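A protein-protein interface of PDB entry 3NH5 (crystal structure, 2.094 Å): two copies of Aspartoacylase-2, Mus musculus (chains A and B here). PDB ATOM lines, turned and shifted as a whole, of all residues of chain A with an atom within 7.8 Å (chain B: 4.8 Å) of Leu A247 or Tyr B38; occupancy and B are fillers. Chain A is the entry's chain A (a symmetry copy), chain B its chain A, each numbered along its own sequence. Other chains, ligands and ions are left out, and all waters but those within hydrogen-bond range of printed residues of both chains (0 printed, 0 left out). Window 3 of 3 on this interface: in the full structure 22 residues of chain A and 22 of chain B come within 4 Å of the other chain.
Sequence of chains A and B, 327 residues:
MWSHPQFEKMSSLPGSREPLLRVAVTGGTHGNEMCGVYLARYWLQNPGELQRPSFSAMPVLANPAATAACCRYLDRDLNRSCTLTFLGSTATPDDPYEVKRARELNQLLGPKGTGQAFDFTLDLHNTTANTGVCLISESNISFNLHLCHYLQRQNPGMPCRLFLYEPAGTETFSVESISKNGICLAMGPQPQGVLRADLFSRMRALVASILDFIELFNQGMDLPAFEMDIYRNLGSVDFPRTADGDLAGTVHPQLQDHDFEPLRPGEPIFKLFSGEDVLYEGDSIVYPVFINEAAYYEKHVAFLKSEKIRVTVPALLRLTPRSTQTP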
ATOM      1  N   ASP A 238     -13.260  13.595  -5.637  1.00  0.00           N
ATOM      2  CA  ASP A 238     -13.295  15.047  -5.657  1.00  0.00           C
ATOM      3  C   ASP A 238     -13.491  15.608  -4.252  1.00  0.00           C
ATOM      4  O   ASP A 238     -13.877  14.880  -3.333  1.00  0.00           O
ATOM      5  CB  ASP A 238     -14.411  15.541  -6.574  1.00  0.00           C
ATOM      6  CG  ASP A 238     -14.361  17.037  -6.793  1.00  0.00           C
ATOM      7  OD1 ASP A 238     -13.326  17.667  -6.457  1.00  0.00           O
ATOM      8  OD2 ASP A 238     -15.351  17.584  -7.326  1.00  0.00           O
ATOM      9  N   PHE A 239     -13.198  16.896  -4.090  1.00  0.00           N
ATOM     10  CA  PHE A 239     -13.430  17.585  -2.827  1.00  0.00           C
ATOM     11  C   PHE A 239     -14.924  17.647  -2.574  1.00  0.00           C
ATOM     12  O   PHE A 239     -15.703  17.766  -3.521  1.00  0.00           O
ATOM     13  CB  PHE A 239     -12.901  19.022  -2.885  1.00  0.00           C
ATOM     14  CG  PHE A 239     -11.405  19.130  -2.830  1.00  0.00           C
ATOM     15  CD1 PHE A 239     -10.653  19.108  -3.994  1.00  0.00           C
ATOM     16  CD2 PHE A 239     -10.747  19.268  -1.612  1.00  0.00           C
ATOM     17  CE1 PHE A 239      -9.261  19.215  -3.947  1.00  0.00           C
ATOM     18  CE2 PHE A 239      -9.360  19.381  -1.557  1.00  0.00           C
ATOM     19  CZ  PHE A 239      -8.619  19.359  -2.731  1.00  0.00           C
ATOM     20  N   PRO A 240     -15.329  17.605  -1.292  1.00  0.00           N
ATOM     21  CA  PRO A 240     -16.740  17.860  -0.966  1.00  0.00           C
ATOM     22  C   PRO A 240     -17.105  19.229  -1.517  1.00  0.00           C
ATOM     23  O   PRO A 240     -16.334  20.172  -1.335  1.00  0.00           O
ATOM     24  CB  PRO A 240     -16.752  17.921   0.567  1.00  0.00           C
ATOM     25  CG  PRO A 240     -15.452  17.370   1.023  1.00  0.00           C
ATOM     26  CD  PRO A 240     -14.468  17.569  -0.097  1.00  0.00           C
ATOM     27  N   ARG A 241     -18.236  19.352  -2.194  1.00  0.00           N
ATOM     28  CA  ARG A 241     -18.609  20.653  -2.736  1.00  0.00           C
ATOM     29  C   ARG A 241     -20.039  21.086  -2.407  1.00  0.00           C
ATOM     30  O   ARG A 241     -20.893  20.271  -2.037  1.00  0.00           O
ATOM     31  CB  ARG A 241     -18.358  20.706  -4.243  1.00  0.00           C
ATOM     32  CG  ARG A 241     -16.904  20.430  -4.608  1.00  0.00           C
ATOM     33  CD  ARG A 241     -16.606  20.725  -6.065  1.00  0.00           C
ATOM     34  NE  ARG A 241     -15.240  20.350  -6.405  1.00  0.00           N
ATOM     35  CZ  ARG A 241     -14.219  21.200  -6.465  1.00  0.00           C
ATOM     36  NH1 ARG A 241     -14.405  22.488  -6.219  1.00  0.00           N
ATOM     37  NH2 ARG A 241     -13.012  20.760  -6.776  1.00  0.00           N
ATOM     38  N   THR A 242     -20.272  22.389  -2.515  1.00  0.00           N
ATOM     39  CA  THR A 242     -21.607  22.941  -2.395  1.00  0.00           C
ATOM     40  C   THR A 242     -22.319  22.622  -3.698  1.00  0.00           C
ATOM     41  O   THR A 242     -21.706  22.086  -4.624  1.00  0.00           O
ATOM     42  CB  THR A 242     -21.561  24.467  -2.214  1.00  0.00           C
ATOM     43  OG1 THR A 242     -20.991  25.067  -3.383  1.00  0.00           O
ATOM     44  CG2 THR A 242     -20.723  24.843  -0.996  1.00  0.00           C
ATOM     45  N   ASP A 244     -22.799  24.525  -5.766  1.00  0.00           N
ATOM     46  CA  ASP A 244     -22.150  25.411  -6.733  1.00  0.00           C
ATOM     47  C   ASP A 244     -20.720  24.998  -7.055  1.00  0.00           C
ATOM     48  O   ASP A 244     -19.986  25.738  -7.716  1.00  0.00           O
ATOM     49  CB  ASP A 244     -22.169  26.863  -6.247  1.00  0.00           C
ATOM     50  CG  ASP A 244     -23.518  27.508  -6.423  1.00  0.00           C
ATOM     51  OD1 ASP A 244     -24.438  26.810  -6.908  1.00  0.00           O
ATOM     52  OD2 ASP A 244     -23.659  28.706  -6.080  1.00  0.00           O
ATOM     53  N   GLY A 245     -20.324  23.821  -6.580  1.00  0.00           N
ATOM     54  CA  GLY A 245     -18.997  23.301  -6.858  1.00  0.00           C
ATOM     55  C   GLY A 245     -17.866  24.064  -6.183  1.00  0.00           C
ATOM     56  O   GLY A 245     -16.698  23.923  -6.561  1.00  0.00           O
ATOM     57  N   ASP A 246     -18.206  24.878  -5.190  1.00  0.00           N
ATOM     58  CA  ASP A 246     -17.190  25.516  -4.365  1.00  0.00           C
ATOM     59  C   ASP A 246     -16.870  24.556  -3.233  1.00  0.00           C
ATOM     60  O   ASP A 246     -17.720  23.766  -2.833  1.00  0.00           O
ATOM     61  CB  ASP A 246     -17.703  26.835  -3.794  1.00  0.00           C
ATOM     62  CG  ASP A 246     -18.474  27.648  -4.810  1.00  0.00           C
ATOM     63  OD1 ASP A 246     -17.847  28.139  -5.776  1.00  0.00           O
ATOM     64  OD2 ASP A 246     -19.706  27.798  -4.633  1.00  0.00           O
ATOM     65  N   LEU A 247     -15.647  24.611  -2.720  1.00  0.00           N
ATOM     66  CA  LEU A 247     -15.287  23.732  -1.624  1.00  0.00           C
ATOM     67  C   LEU A 247     -16.281  23.885  -0.482  1.00  0.00           C
ATOM     68  O   LEU A 247     -16.662  25.001  -0.126  1.00  0.00           O
ATOM     69  CB  LEU A 247     -13.886  24.045  -1.098  1.00  0.00           C
ATOM     70  CG  LEU A 247     -12.648  23.824  -1.964  1.00  0.00           C
ATOM     71  CD1 LEU A 247     -11.412  23.836  -1.066  1.00  0.00           C
ATOM     72  CD2 LEU A 247     -12.712  22.534  -2.726  1.00  0.00           C
ATOM     73  N   ALA A 248     -16.682  22.763   0.100  1.00  0.00           N
ATOM     74  CA  ALA A 248     -17.466  22.787   1.322  1.00  0.00           C
ATOM     75  C   ALA A 248     -16.622  22.178   2.433  1.00  0.00           C
ATOM     76  O   ALA A 248     -17.054  22.058   3.586  1.00  0.00           O
ATOM     77  CB  ALA A 248     -18.763  22.011   1.133  1.00  0.00           C
ATOM     78  N   GLY A 249     -15.402  21.794   2.071  1.00  0.00           N
ATOM     79  CA  GLY A 249     -14.461  21.239   3.024  1.00  0.00           C
ATOM     80  C   GLY A 249     -13.129  20.960   2.351  1.00  0.00           C
ATOM     81  O   GLY A 249     -12.951  21.233   1.164  1.00  0.00           O
ATOM     82  N   THR A 250     -12.186  20.417   3.109  1.00  0.00           N
ATOM     83  CA  THR A 250     -10.927  19.990   2.514  1.00  0.00           C
ATOM     84  C   THR A 250     -10.491  18.636   3.066  1.00  0.00           C
ATOM     85  O   THR A 250     -11.193  18.015   3.878  1.00  0.00           O
ATOM     86  CB  THR A 250      -9.800  21.042   2.670  1.00  0.00           C
ATOM     87  OG1 THR A 250      -8.683  20.683   1.840  1.00  0.00           O
ATOM     88  CG2 THR A 250      -9.362  21.166   4.128  1.00  0.00           C
ATOM     89  N   VAL A 251      -9.339  18.175   2.592  1.00  0.00           N
ATOM     90  CA  VAL A 251      -8.817  16.875   2.966  1.00  0.00           C
ATOM     91  C   VAL A 251      -8.673  16.791   4.483  1.00  0.00           C
ATOM     92  O   VAL A 251      -8.116  17.689   5.122  1.00  0.00           O
ATOM     93  CB  VAL A 251      -7.449  16.606   2.257  1.00  0.00           C
ATOM     94  CG1 VAL A 251      -6.819  15.309   2.750  1.00  0.00           C
ATOM     95  CG2 VAL A 251      -7.640  16.584   0.731  1.00  0.00           C
ATOM     96  N   LEU A 272     -15.483  18.884   6.638  1.00  0.00           N
ATOM     97  CA  LEU A 272     -16.299  19.976   6.116  1.00  0.00           C
ATOM     98  C   LEU A 272     -16.142  21.229   6.975  1.00  0.00           C
ATOM     99  O   LEU A 272     -15.853  21.139   8.166  1.00  0.00           O
ATOM    100  CB  LEU A 272     -17.765  19.564   6.090  1.00  0.00           C
ATOM    101  CG  LEU A 272     -18.099  18.302   5.313  1.00  0.00           C
ATOM    102  CD1 LEU A 272     -19.596  18.070   5.372  1.00  0.00           C
ATOM    103  CD2 LEU A 272     -17.629  18.451   3.883  1.00  0.00           C
ATOM    104  N   PHE A 273     -16.334  22.399   6.381  1.00  0.00           N
ATOM    105  CA  PHE A 273     -16.222  23.631   7.153  1.00  0.00           C
ATOM    106  C   PHE A 273     -17.257  23.644   8.297  1.00  0.00           C
ATOM    107  O   PHE A 273     -17.038  24.258   9.343  1.00  0.00           O
ATOM    108  CB  PHE A 273     -16.381  24.861   6.250  1.00  0.00           C
ATOM    109  CG  PHE A 273     -15.406  24.906   5.110  1.00  0.00           C
ATOM    110  CD1 PHE A 273     -14.090  24.496   5.288  1.00  0.00           C
ATOM    111  CD2 PHE A 273     -15.797  25.353   3.863  1.00  0.00           C
ATOM    112  CE1 PHE A 273     -13.185  24.532   4.241  1.00  0.00           C
ATOM    113  CE2 PHE A 273     -14.890  25.397   2.796  1.00  0.00           C
ATOM    114  CZ  PHE A 273     -13.585  24.991   2.990  1.00  0.00           C
ATOM    115  N   ASN A 292      -4.340  16.233  -1.979  1.00  0.00           N
ATOM    116  CA  ASN A 292      -4.302  17.698  -1.836  1.00  0.00           C
ATOM    117  C   ASN A 292      -3.190  18.366  -2.669  1.00  0.00           C
ATOM    118  O   ASN A 292      -2.339  19.071  -2.128  1.00  0.00           O
ATOM    119  CB  ASN A 292      -4.200  18.114  -0.356  1.00  0.00           C
ATOM    120  CG  ASN A 292      -5.012  19.382  -0.031  1.00  0.00           C
ATOM    121  OD1 ASN A 292      -5.565  20.029  -0.923  1.00  0.00           O
ATOM    122  ND2 ASN A 292      -5.075  19.738   1.253  1.00  0.00           N
ATOM    123  N   TYR A 297      -7.149  20.920  -7.755  1.00  0.00           N
ATOM    124  CA  TYR A 297      -8.406  21.545  -7.317  1.00  0.00           C
ATOM    125  C   TYR A 297      -9.348  21.751  -8.507  1.00  0.00           C
ATOM    126  O   TYR A 297     -10.489  21.274  -8.493  1.00  0.00           O
ATOM    127  CB  TYR A 297      -8.138  22.878  -6.608  1.00  0.00           C
ATOM    128  CG  TYR A 297      -7.756  22.727  -5.144  1.00  0.00           C
ATOM    129  CD1 TYR A 297      -6.612  22.031  -4.771  1.00  0.00           C
ATOM    130  CD2 TYR A 297      -8.538  23.291  -4.140  1.00  0.00           C
ATOM    131  CE1 TYR A 297      -6.255  21.894  -3.443  1.00  0.00           C
ATOM    132  CE2 TYR A 297      -8.187  23.153  -2.794  1.00  0.00           C
ATOM    133  CZ  TYR A 297      -7.046  22.455  -2.459  1.00  0.00           C
ATOM    134  OH  TYR A 297      -6.695  22.301  -1.143  1.00  0.00           O
ATOM    135  N   HIS A 300     -10.946  18.902 -10.197  1.00  0.00           N
ATOM    136  CA  HIS A 300     -11.874  18.191  -9.320  1.00  0.00           C
ATOM    137  C   HIS A 300     -11.302  16.896  -8.757  1.00  0.00           C
ATOM    138  O   HIS A 300     -11.989  15.879  -8.722  1.00  0.00           O
ATOM    139  CB  HIS A 300     -13.201  17.944 -10.045  1.00  0.00           C
ATOM    140  CG  HIS A 300     -13.983  19.197 -10.268  1.00  0.00           C
ATOM    141  ND1 HIS A 300     -15.035  19.571  -9.459  1.00  0.00           N
ATOM    142  CD2 HIS A 300     -13.828  20.195 -11.170  1.00  0.00           C
ATOM    143  CE1 HIS A 300     -15.512  20.733  -9.871  1.00  0.00           C
ATOM    144  NE2 HIS A 300     -14.798  21.133 -10.908  1.00  0.00           N
ATOM    145  N   ALA A 302      -9.283  15.559  -5.308  1.00  0.00           N
ATOM    146  CA  ALA A 302      -8.721  15.719  -3.974  1.00  0.00           C
ATOM    147  C   ALA A 302      -7.646  14.666  -3.781  1.00  0.00           C
ATOM    148  O   ALA A 302      -6.670  14.867  -3.059  1.00  0.00           O
ATOM    149  CB  ALA A 302      -9.825  15.571  -2.899  1.00  0.00           C
ATOM    150  N   MET B  34      -4.960  30.300   0.973  1.00  0.00           N
ATOM    151  CA  MET B  34      -6.266  29.668   1.018  1.00  0.00           C
ATOM    152  C   MET B  34      -7.032  29.733   2.331  1.00  0.00           C
ATOM    153  O   MET B  34      -8.248  29.590   2.321  1.00  0.00           O
ATOM    154  CB  MET B  34      -6.167  28.201   0.550  1.00  0.00           C
ATOM    155  CG  MET B  34      -5.502  28.056  -0.820  1.00  0.00           C
ATOM    156  SD  MET B  34      -6.475  28.896  -2.081  1.00  0.00           S
ATOM    157  CE  MET B  34      -7.576  27.558  -2.535  1.00  0.00           C
ATOM    158  N   CYS B  35      -6.358  29.898   3.460  1.00  0.00           N
ATOM    159  CA  CYS B  35      -7.124  29.920   4.712  1.00  0.00           C
ATOM    160  C   CYS B  35      -8.019  31.154   4.719  1.00  0.00           C
ATOM    161  O   CYS B  35      -9.228  31.052   4.938  1.00  0.00           O
ATOM    162  CB  CYS B  35      -6.221  29.909   5.950  1.00  0.00           C
ATOM    163  SG  CYS B  35      -5.328  28.343   6.208  1.00  0.00           S
ATOM    164  N   GLY B  36      -7.410  32.307   4.455  1.00  0.00           N
ATOM    165  CA  GLY B  36      -8.120  33.571   4.457  1.00  0.00           C
ATOM    166  C   GLY B  36      -9.205  33.582   3.396  1.00  0.00           C
ATOM    167  O   GLY B  36     -10.310  34.076   3.633  1.00  0.00           O
ATOM    168  N   VAL B  37      -8.887  33.039   2.224  1.00  0.00           N
ATOM    169  CA  VAL B  37      -9.848  32.966   1.135  1.00  0.00           C
ATOM    170  C   VAL B  37     -11.109  32.223   1.587  1.00  0.00           C
ATOM    171  O   VAL B  37     -12.230  32.728   1.452  1.00  0.00           O
ATOM    172  CB  VAL B  37      -9.261  32.255  -0.112  1.00  0.00           C
ATOM    173  CG1 VAL B  37     -10.372  31.808  -1.032  1.00  0.00           C
ATOM    174  CG2 VAL B  37      -8.305  33.158  -0.851  1.00  0.00           C
ATOM    175  N   TYR B  38     -10.930  31.038   2.158  1.00  0.00           N
ATOM    176  CA  TYR B  38     -12.089  30.210   2.481  1.00  0.00           C
ATOM    177  C   TYR B  38     -12.789  30.591   3.775  1.00  0.00           C
ATOM    178  O   TYR B  38     -13.981  30.338   3.932  1.00  0.00           O
ATOM    179  CB  TYR B  38     -11.755  28.699   2.391  1.00  0.00           C
ATOM    180  CG  TYR B  38     -11.840  28.247   0.954  1.00  0.00           C
ATOM    181  CD1 TYR B  38     -13.071  28.016   0.363  1.00  0.00           C
ATOM    182  CD2 TYR B  38     -10.703  28.151   0.161  1.00  0.00           C
ATOM    183  CE1 TYR B  38     -13.173  27.643  -0.960  1.00  0.00           C
ATOM    184  CE2 TYR B  38     -10.799  27.771  -1.174  1.00  0.00           C
ATOM    185  CZ  TYR B  38     -12.039  27.522  -1.723  1.00  0.00           C
ATOM    186  OH  TYR B  38     -12.159  27.153  -3.044  1.00  0.00           O
ATOM    187  N   LEU B  39     -12.058  31.210   4.694  1.00  0.00           N
ATOM    188  CA  LEU B  39     -12.678  31.730   5.899  1.00  0.00           C
ATOM    189  C   LEU B  39     -13.571  32.923   5.537  1.00  0.00           C
ATOM    190  O   LEU B  39     -14.720  32.970   5.952  1.00  0.00           O
ATOM    191  CB  LEU B  39     -11.637  32.114   6.950  1.00  0.00           C
ATOM    192  CG  LEU B  39     -11.000  30.931   7.693  1.00  0.00           C
ATOM    193  CD1 LEU B  39      -9.806  31.401   8.512  1.00  0.00           C
ATOM    194  CD2 LEU B  39     -12.021  30.202   8.569  1.00  0.00           C
ATOM    195  N   ALA B  40     -13.045  33.858   4.746  1.00  0.00           N
ATOM    196  CA  ALA B  40     -13.850  34.981   4.251  1.00  0.00           C
ATOM    197  C   ALA B  40     -15.102  34.513   3.489  1.00  0.00           C
ATOM    198  O   ALA B  40     -16.207  34.982   3.766  1.00  0.00           O
ATOM    199  CB  ALA B  40     -13.005  35.903   3.375  1.00  0.00           C
ATOM    200  N   ARG B  41     -14.933  33.595   2.531  1.00  0.00           N
ATOM    201  CA  ARG B  41     -16.080  33.058   1.780  1.00  0.00           C
ATOM    202  C   ARG B  41     -17.094  32.395   2.704  1.00  0.00           C
ATOM    203  O   ARG B  41     -18.304  32.560   2.550  1.00  0.00           O
ATOM    204  CB  ARG B  41     -15.627  32.053   0.716  1.00  0.00           C
ATOM    205  CG  ARG B  41     -15.078  32.692  -0.547  1.00  0.00           C
ATOM    206  CD  ARG B  41     -14.486  31.644  -1.472  1.00  0.00           C
ATOM    207  NE  ARG B  41     -14.136  32.187  -2.784  1.00  0.00           N
ATOM    208  CZ  ARG B  41     -13.523  31.494  -3.736  1.00  0.00           C
ATOM    209  NH1 ARG B  41     -13.170  30.231  -3.522  1.00  0.00           N
ATOM    210  NH2 ARG B  41     -13.258  32.059  -4.903  1.00  0.00           N
ATOM    211  N   TYR B  42     -16.594  31.647   3.677  1.00  0.00           N
ATOM    212  CA  TYR B  42     -17.471  30.969   4.606  1.00  0.00           C
ATOM    213  C   TYR B  42     -18.218  31.974   5.490  1.00  0.00           C
ATOM    214  O   TYR B  42     -19.425  31.847   5.696  1.00  0.00           O
ATOM    215  CB  TYR B  42     -16.668  30.008   5.474  1.00  0.00           C
ATOM    216  CG  TYR B  42     -17.500  29.283   6.495  1.00  0.00           C
ATOM    217  CD1 TYR B  42     -18.244  28.164   6.138  1.00  0.00           C
ATOM    218  CD2 TYR B  42     -17.554  29.719   7.810  1.00  0.00           C
ATOM    219  CE1 TYR B  42     -19.014  27.495   7.059  1.00  0.00           C
ATOM    220  CE2 TYR B  42     -18.331  29.051   8.752  1.00  0.00           C
ATOM    221  CZ  TYR B  42     -19.054  27.935   8.366  1.00  0.00           C
ATOM    222  OH  TYR B  42     -19.828  27.252   9.282  1.00  0.00           O
ATOM    223  N   LEU B 195      -5.448  24.230   0.547  1.00  0.00           N
ATOM    224  CA  LEU B 195      -6.094  24.428   1.834  1.00  0.00           C
ATOM    225  C   LEU B 195      -5.885  23.206   2.713  1.00  0.00           C
ATOM    226  O   LEU B 195      -6.430  22.130   2.443  1.00  0.00           O
ATOM    227  CB  LEU B 195      -7.611  24.662   1.654  1.00  0.00           C
ATOM    228  CG  LEU B 195      -8.388  24.956   2.943  1.00  0.00           C
ATOM    229  CD1 LEU B 195      -7.840  26.226   3.599  1.00  0.00           C
ATOM    230  CD2 LEU B 195      -9.881  25.112   2.692  1.00  0.00           C
ATOM    231  N   PHE B 200      -6.563  25.660   8.487  1.00  0.00           N
ATOM    232  CA  PHE B 200      -7.867  26.296   8.412  1.00  0.00           C
ATOM    233  C   PHE B 200      -8.505  26.373   9.810  1.00  0.00           C
ATOM    234  O   PHE B 200      -8.912  27.450  10.243  1.00  0.00           O
ATOM    235  CB  PHE B 200      -8.766  25.536   7.449  1.00  0.00           C
ATOM    236  CG  PHE B 200     -10.150  26.121   7.302  1.00  0.00           C
ATOM    237  CD1 PHE B 200     -10.373  27.216   6.464  1.00  0.00           C
ATOM    238  CD2 PHE B 200     -11.232  25.562   7.981  1.00  0.00           C
ATOM    239  CE1 PHE B 200     -11.668  27.748   6.306  1.00  0.00           C
ATOM    240  CE2 PHE B 200     -12.522  26.087   7.835  1.00  0.00           C
ATOM    241  CZ  PHE B 200     -12.738  27.177   6.999  1.00  0.00           C
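Among the printed residues, merely in contact across the chains: Leu A247 with Tyr B38 (3.5 Å), Phe A273 with Tyr B42 (3.8 Å), Phe A273 with Leu B195 (3.7 Å) and Phe A273 with Phe B200 (3.4 Å).
No position is printed for both chains.
Of the 7 pairs that touch across the chains among the printed residues, none has its exchanged pair printed and touching as well.
The backbone NH of Phe B200 is in hydrogen-bond range of the side-chain sulfur of Cys B35 (3.7 Å).
The backbone NH (N) of Asn A292 sits at hydrogen-bond distance from the backbone carbonyl oxygen (O) of Ala A302 (2.9 Å).
The backbone carbonyl oxygen (O) of Tyr A297 lies within hydrogen-bond range of the guanidinium group (NH2) of Arg A241 (3.1 Å).
The side-chain hydroxyl (OH) of Tyr B38 lies within hydrogen-bond range of the guanidinium group (NH1) of Arg B41.
The backbone carbonyl oxygen (O) of Ala A248 sits at hydrogen-bond distance from the backbone NH (N) of Phe A273.
The side-chain amide oxygen of Asn A292 is in hydrogen-bond range of the side-chain hydroxyl of Tyr A297 (2.5 Å).
Pro A240 touches none of the printed residues of chain B.
Of chain B, only Tyr B38 (3.5 Å) comes within 4 Å of Leu A247.
Printed residues of chain B within 4 Å of Thr A250: Leu B195 (2.7 Å).
Printed residues of chain B within 4 Å of Phe A273: Tyr B42, Leu B195 and Phe B200.
Printed residues of chain B within 4 Å of Tyr A297: Leu B195 (2.9 Å).
Cys B35 touches none of the printed residues of chain A.
Of the printed residues of chain A, Tyr B38 touches Leu A247.
Of the printed residues of chain A, Tyr B42 touches Phe A273 (3.8 Å).
Of the printed residues of chain A, Leu B195 touches Thr A250 (2.7 Å), Phe A273 (3.7 Å), Asn A292 (3.0 Å) and Tyr A297 (2.9 Å).
Of the 11 printed residues of chain B, 4 touch a printed residue of chain A.
Hydrophobic or aromatic side chains of chain A that line the printed part of chain B: Leu A247, Phe A273 and Tyr A297.
Among the printed residues, 7 pairs touch across the chains.
Among the printed residues, no Asp or Glu carboxylate lies within 4 Å of a Lys or Arg side-chain nitrogen of the other chain.
O of Leu B195 lies within hydrogen-bond range of OG1 of Thr A250 (2.7 Å).
The side-chain amide nitrogen (ND2) of Asn A292 is in hydrogen-bond range of the backbone carbonyl oxygen (O) of Leu B195.
N of Leu B195 is in hydrogen-bond range of OH of Tyr A297.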
